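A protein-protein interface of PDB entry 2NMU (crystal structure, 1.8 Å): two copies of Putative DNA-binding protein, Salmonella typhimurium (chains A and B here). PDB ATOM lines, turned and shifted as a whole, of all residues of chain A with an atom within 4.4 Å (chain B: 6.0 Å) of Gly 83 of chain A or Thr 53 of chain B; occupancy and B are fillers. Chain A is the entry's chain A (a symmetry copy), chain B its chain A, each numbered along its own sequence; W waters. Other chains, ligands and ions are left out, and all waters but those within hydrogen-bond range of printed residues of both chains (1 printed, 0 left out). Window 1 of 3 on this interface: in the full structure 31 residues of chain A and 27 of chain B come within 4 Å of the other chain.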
ATOM      1  N   TRP A  48     -22.631  -8.728  -5.168  1.00  0.00           N
ATOM      2  CA  TRP A  48     -23.111  -8.722  -6.545  1.00  0.00           C
ATOM      3  C   TRP A  48     -24.418  -9.492  -6.601  1.00  0.00           C
ATOM      4  O   TRP A  48     -24.704 -10.307  -5.723  1.00  0.00           O
ATOM      5  CB  TRP A  48     -22.069  -9.343  -7.492  1.00  0.00           C
ATOM      6  CG  TRP A  48     -22.143 -10.838  -7.682  1.00  0.00           C
ATOM      7  CD1 TRP A  48     -22.776 -11.508  -8.694  1.00  0.00           C
ATOM      8  CD2 TRP A  48     -21.530 -11.841  -6.861  1.00  0.00           C
ATOM      9  NE1 TRP A  48     -22.591 -12.862  -8.557  1.00  0.00           N
ATOM     10  CE2 TRP A  48     -21.832 -13.097  -7.442  1.00  0.00           C
ATOM     11  CE3 TRP A  48     -20.753 -11.802  -5.692  1.00  0.00           C
ATOM     12  CZ2 TRP A  48     -21.386 -14.308  -6.895  1.00  0.00           C
ATOM     13  CZ3 TRP A  48     -20.306 -13.007  -5.148  1.00  0.00           C
ATOM     14  CH2 TRP A  48     -20.627 -14.246  -5.754  1.00  0.00           C
ATOM     15  N   ILE A  49     -25.230  -9.222  -7.614  1.00  0.00           N
ATOM     16  CA  ILE A  49     -26.496  -9.934  -7.742  1.00  0.00           C
ATOM     17  C   ILE A  49     -26.205 -11.271  -8.411  1.00  0.00           C
ATOM     18  O   ILE A  49     -25.869 -11.326  -9.598  1.00  0.00           O
ATOM     19  CB  ILE A  49     -27.505  -9.145  -8.596  1.00  0.00           C
ATOM     20  CG1 ILE A  49     -27.604  -7.703  -8.084  1.00  0.00           C
ATOM     21  CG2 ILE A  49     -28.880  -9.823  -8.525  1.00  0.00           C
ATOM     22  CD1 ILE A  49     -28.085  -7.590  -6.653  1.00  0.00           C
ATOM     23  N   ASN A  82     -28.456  -7.484 -13.045  1.00  0.00           N
ATOM     24  CA  ASN A  82     -27.051  -7.791 -12.823  1.00  0.00           C
ATOM     25  C   ASN A  82     -26.227  -6.617 -12.333  1.00  0.00           C
ATOM     26  O   ASN A  82     -26.573  -5.458 -12.553  1.00  0.00           O
ATOM     27  CB  ASN A  82     -26.436  -8.298 -14.126  1.00  0.00           C
ATOM     28  CG  ASN A  82     -26.771  -9.743 -14.407  1.00  0.00           C
ATOM     29  OD1 ASN A  82     -26.264 -10.645 -13.739  1.00  0.00           O
ATOM     30  ND2 ASN A  82     -27.622  -9.976 -15.399  1.00  0.00           N
ATOM     31  N   GLY A  83     -25.121  -6.920 -11.668  1.00  0.00           N
ATOM     32  CA  GLY A  83     -24.269  -5.850 -11.202  1.00  0.00           C
ATOM     33  C   GLY A  83     -23.685  -6.037  -9.827  1.00  0.00           C
ATOM     34  O   GLY A  83     -23.930  -7.027  -9.131  1.00  0.00           O
ATOM     35  N   THR A  84     -22.900  -5.049  -9.435  1.00  0.00           N
ATOM     36  CA  THR A  84     -22.227  -5.061  -8.151  1.00  0.00           C
ATOM     37  C   THR A  84     -22.809  -3.994  -7.240  1.00  0.00           C
ATOM     38  O   THR A  84     -23.446  -3.045  -7.698  1.00  0.00           O
ATOM     39  CB  THR A  84     -20.740  -4.756  -8.340  1.00  0.00           C
ATOM     40  OG1 THR A  84     -20.614  -3.511  -9.039  1.00  0.00           O
ATOM     41  CG2 THR A  84     -20.059  -5.855  -9.153  1.00  0.00           C
ATOM     42  N   HIS A  91     -23.606  -0.549  -9.199  1.00  0.00           N
ATOM     43  CA  HIS A  91     -23.643  -0.430 -10.646  1.00  0.00           C
ATOM     44  C   HIS A  91     -24.491  -1.607 -11.099  1.00  0.00           C
ATOM     45  O   HIS A  91     -23.995  -2.726 -11.244  1.00  0.00           O
ATOM     46  CB  HIS A  91     -22.230  -0.529 -11.226  1.00  0.00           C
ATOM     47  CG  HIS A  91     -22.163  -0.300 -12.703  1.00  0.00           C
ATOM     48  ND1 HIS A  91     -20.982  -0.354 -13.411  1.00  0.00           N
ATOM     49  CD2 HIS A  91     -23.130  -0.020 -13.609  1.00  0.00           C
ATOM     50  CE1 HIS A  91     -21.225  -0.119 -14.688  1.00  0.00           C
ATOM     51  NE2 HIS A  91     -22.521   0.087 -14.835  1.00  0.00           N
ATOM     52  N   LEU A  92     -25.775  -1.345 -11.315  1.00  0.00           N
ATOM     53  CA  LEU A  92     -26.719  -2.387 -11.705  1.00  0.00           C
ATOM     54  C   LEU A  92     -27.410  -2.140 -13.039  1.00  0.00           C
ATOM     55  O   LEU A  92     -27.744  -1.005 -13.376  1.00  0.00           O
ATOM     56  CB  LEU A  92     -27.782  -2.526 -10.614  1.00  0.00           C
ATOM     57  CG  LEU A  92     -27.226  -2.810  -9.213  1.00  0.00           C
ATOM     58  CD1 LEU A  92     -28.287  -2.520  -8.161  1.00  0.00           C
ATOM     59  CD2 LEU A  92     -26.748  -4.252  -9.138  1.00  0.00           C
ATOM     60  N   HIS A  93     -27.614  -3.214 -13.797  1.00  0.00           N
ATOM     61  CA  HIS A  93     -28.299  -3.137 -15.082  1.00  0.00           C
ATOM     62  C   HIS A  93     -29.546  -3.999 -14.989  1.00  0.00           C
ATOM     63  O   HIS A  93     -29.529  -5.055 -14.358  1.00  0.00           O
ATOM     64  CB  HIS A  93     -27.399  -3.636 -16.217  1.00  0.00           C
ATOM     65  CG  HIS A  93     -26.326  -2.667 -16.603  1.00  0.00           C
ATOM     66  ND1 HIS A  93     -25.656  -2.740 -17.804  1.00  0.00           N
ATOM     67  CD2 HIS A  93     -25.823  -1.589 -15.957  1.00  0.00           C
ATOM     68  CE1 HIS A  93     -24.788  -1.748 -17.884  1.00  0.00           C
ATOM     69  NE2 HIS A  93     -24.869  -1.036 -16.777  1.00  0.00           N
ATOM     70  N   GLY B  51     -21.557 -12.961 -12.590  1.00  0.00           N
ATOM     71  CA  GLY B  51     -22.153 -11.633 -12.591  1.00  0.00           C
ATOM     72  C   GLY B  51     -21.399 -10.717 -13.534  1.00  0.00           C
ATOM     73  O   GLY B  51     -20.187 -10.839 -13.664  1.00  0.00           O
ATOM     74  N   CYS B  52     -22.101  -9.801 -14.193  1.00  0.00           N
ATOM     75  CA  CYS B  52     -21.436  -8.899 -15.130  1.00  0.00           C
ATOM     76  C   CYS B  52     -22.257  -7.662 -15.451  1.00  0.00           C
ATOM     77  O   CYS B  52     -23.473  -7.736 -15.609  1.00  0.00           O
ATOM     78  CB  CYS B  52     -21.131  -9.647 -16.435  1.00  0.00           C
ATOM     79  SG  CYS B  52     -20.353  -8.662 -17.756  1.00  0.00           S
ATOM     80  N   THR B  53     -21.579  -6.525 -15.545  1.00  0.00           N
ATOM     81  CA  THR B  53     -22.227  -5.268 -15.884  1.00  0.00           C
ATOM     82  C   THR B  53     -21.181  -4.375 -16.541  1.00  0.00           C
ATOM     83  O   THR B  53     -19.998  -4.465 -16.221  1.00  0.00           O
ATOM     84  CB  THR B  53     -22.800  -4.559 -14.634  1.00  0.00           C
ATOM     85  OG1 THR B  53     -23.535  -3.401 -15.043  1.00  0.00           O
ATOM     86  CG2 THR B  53     -21.691  -4.127 -13.692  1.00  0.00           C
ATOM     87  N   GLY B  54     -21.611  -3.525 -17.466  1.00  0.00           N
ATOM     88  CA  GLY B  54     -20.668  -2.646 -18.130  1.00  0.00           C
ATOM     89  C   GLY B  54     -21.172  -2.088 -19.444  1.00  0.00           C
ATOM     90  O   GLY B  54     -22.375  -2.049 -19.694  1.00  0.00           O
ATOM     91  N   SER B  55     -20.245  -1.671 -20.296  1.00  0.00           N
ATOM     92  CA  SER B  55     -20.604  -1.082 -21.583  1.00  0.00           C
ATOM     93  C   SER B  55     -19.640  -1.488 -22.690  1.00  0.00           C
ATOM     94  O   SER B  55     -18.485  -1.813 -22.429  1.00  0.00           O
ATOM     95  CB  SER B  55     -20.618   0.443 -21.452  1.00  0.00           C
ATOM     96  OG  SER B  55     -19.402   0.910 -20.881  1.00  0.00           O
ATOM     97  N   VAL B  78     -24.010  -3.513 -21.466  1.00  0.00           N
ATOM     98  CA  VAL B  78     -24.060  -4.963 -21.356  1.00  0.00           C
ATOM     99  C   VAL B  78     -25.157  -5.263 -20.343  1.00  0.00           C
ATOM    100  O   VAL B  78     -25.046  -4.893 -19.178  1.00  0.00           O
ATOM    101  CB  VAL B  78     -22.740  -5.547 -20.836  1.00  0.00           C
ATOM    102  CG1 VAL B  78     -22.918  -7.033 -20.521  1.00  0.00           C
ATOM    103  CG2 VAL B  78     -21.654  -5.350 -21.873  1.00  0.00           C
ATOM    104  N   THR B 117     -16.306   0.454 -19.132  1.00  0.00           N
ATOM    105  CA  THR B 117     -15.899  -0.542 -18.155  1.00  0.00           C
ATOM    106  C   THR B 117     -16.666  -1.841 -18.346  1.00  0.00           C
ATOM    107  O   THR B 117     -17.695  -1.878 -19.025  1.00  0.00           O
ATOM    108  CB  THR B 117     -16.206  -0.048 -16.719  1.00  0.00           C
ATOM    109  OG1 THR B 117     -15.553  -0.882 -15.754  1.00  0.00           O
ATOM    110  CG2 THR B 117     -17.715  -0.097 -16.459  1.00  0.00           C
ATOM    111  N   LEU B 118     -16.137  -2.905 -17.753  1.00  0.00           N
ATOM    112  CA  LEU B 118     -16.806  -4.202 -17.742  1.00  0.00           C
ATOM    113  C   LEU B 118     -16.432  -4.802 -16.393  1.00  0.00           C
ATOM    114  O   LEU B 118     -15.271  -5.114 -16.137  1.00  0.00           O
ATOM    115  CB  LEU B 118     -16.357  -5.124 -18.880  1.00  0.00           C
ATOM    116  CG  LEU B 118     -17.322  -6.321 -18.987  1.00  0.00           C
ATOM    117  CD1 LEU B 118     -18.669  -5.808 -19.493  1.00  0.00           C
ATOM    118  CD2 LEU B 118     -16.795  -7.397 -19.930  1.00  0.00           C
ATOM    119  N   GLU B 119     -17.423  -4.919 -15.519  1.00  0.00           N
ATOM    120  CA  GLU B 119     -17.222  -5.469 -14.186  1.00  0.00           C
ATOM    121  C   GLU B 119     -17.678  -6.913 -14.222  1.00  0.00           C
ATOM    122  O   GLU B 119     -18.770  -7.212 -14.705  1.00  0.00           O
ATOM    123  CB  GLU B 119     -18.042  -4.680 -13.169  1.00  0.00           C
ATOM    124  CG  GLU B 119     -17.570  -3.249 -12.998  1.00  0.00           C
ATOM    125  CD  GLU B 119     -18.535  -2.402 -12.193  1.00  0.00           C
ATOM    126  OE1 GLU B 119     -19.143  -2.930 -11.238  1.00  0.00           O
ATOM    127  OE2 GLU B 119     -18.673  -1.201 -12.509  1.00  0.00           O
ATOM    128  N   LEU B 120     -16.845  -7.803 -13.702  1.00  0.00           N
ATOM    129  CA  LEU B 120     -17.156  -9.220 -13.723  1.00  0.00           C
ATOM    130  C   LEU B 120     -16.869  -9.944 -12.424  1.00  0.00           C
ATOM    131  O   LEU B 120     -15.917  -9.624 -11.718  1.00  0.00           O
ATOM    132  CB  LEU B 120     -16.331  -9.911 -14.811  1.00  0.00           C
ATOM    133  CG  LEU B 120     -16.514  -9.555 -16.284  1.00  0.00           C
ATOM    134  CD1 LEU B 120     -15.168  -9.588 -16.991  1.00  0.00           C
ATOM    135  CD2 LEU B 120     -17.482 -10.540 -16.916  1.00  0.00           C
HETATM  136  O   HOH W   1     -25.289  -5.900 -16.346  1.00  0.00           O
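O of Val 78 of chain B lies within hydrogen-bond range of ND1 of His 93 of chain A (2.6 Å). OE2 of Glu 119 of chain B lies within hydrogen-bond range of ND1 of His 91 of chain A (2.6 Å). The side-chain hydroxyl (OG1) of Thr 53 of chain B sits close to a ring nitrogen (NE2) of His 93 of chain A, 3.2 Å away. OE1 of Glu 119 of chain B lies within hydrogen-bond range of OG1 of Thr 84 of chain A, at 2.7 Å.
SG of Cys 52 of chain B sits close to O of Glu 119 of chain B (3.7 Å). The backbone NH of His 93 of chain A lies within hydrogen-bond range of the backbone carbonyl oxygen of Asn 82 of chain A (2.8 Å). The backbone carbonyl oxygen (O) of Gly 83 of chain A is in hydrogen-bond range of the backbone NH (N) of Ile 49 of chain A (3.0 Å). The backbone carbonyl oxygen (O) of Thr 53 of chain B sits at hydrogen-bond distance from the backbone NH (N) of Glu 119 of chain B (2.7 Å). N of Val 78 of chain B lies within hydrogen-bond range of O of Gly 54 of chain B (2.8 Å). The backbone NH (N) of Ser 55 of chain B lies within hydrogen-bond range of the backbone carbonyl oxygen (O) of Thr 117 of chain B.
Gly 51 of chain B touches Trp 48 of chain A. O of Cys 52 of chain B touches CB of Asn 82 of chain A, 3.4 Å away. Gly 83 of chain A touches Thr 53 of chain B. NE2 of His 91 of chain A touches OG1 of Thr 53 of chain B (3.6 Å). CE1 of His 91 of chain A touches CG2 of Thr 117 of chain B, 3.9 Å away. His 93 of chain A touches Gly 54 of chain B.
Ile 49 of chain A touches none of the printed residues of chain B. Gly 83 of chain A touches just one residue of chain B: Thr 53. Of the printed residues of chain A, Cys 52 of chain B touches Asn 82 (3.4 Å). Thr 53 of chain B touches just these residues of chain A: Gly 83, His 91 and His 93. Of the printed residues of chain A, Thr 117 of chain B touches His 91 (3.9 Å). Leu 120 of chain B touches none of the printed residues of chain A. The nearest residue of chain B that does not touch Gly 83 of chain A is Cys 52 of chain B (4.3 Å). The nearest printed residue of chain A that does not touch Gly 54 of chain B is His 91 of chain A (4.3 Å).
Of the 10 printed residues of chain B, 7 touch a printed residue of chain A. Of the 8 printed residues of chain A, 6 touch a printed residue of chain B. Among the printed residues, no Asp or Glu carboxylate lies within 4 Å of a Lys or Arg side-chain nitrogen of the other chain.
No position is printed for both chains. Of the 10 pairs that touch across the chains among the printed residues, none has its exchanged pair printed and touching as well.
Water W1 lies within hydrogen-bond range of the backbone carbonyl oxygen of Cys 52 of chain B (2.7 Å), the backbone carbonyl oxygen of Val 78 of chain B (3.0 Å), the side-chain hydroxyl of Thr 53 of chain B (3.3 Å) and a ring nitrogen (ND1) of His 93 of chain A (3.5 Å).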
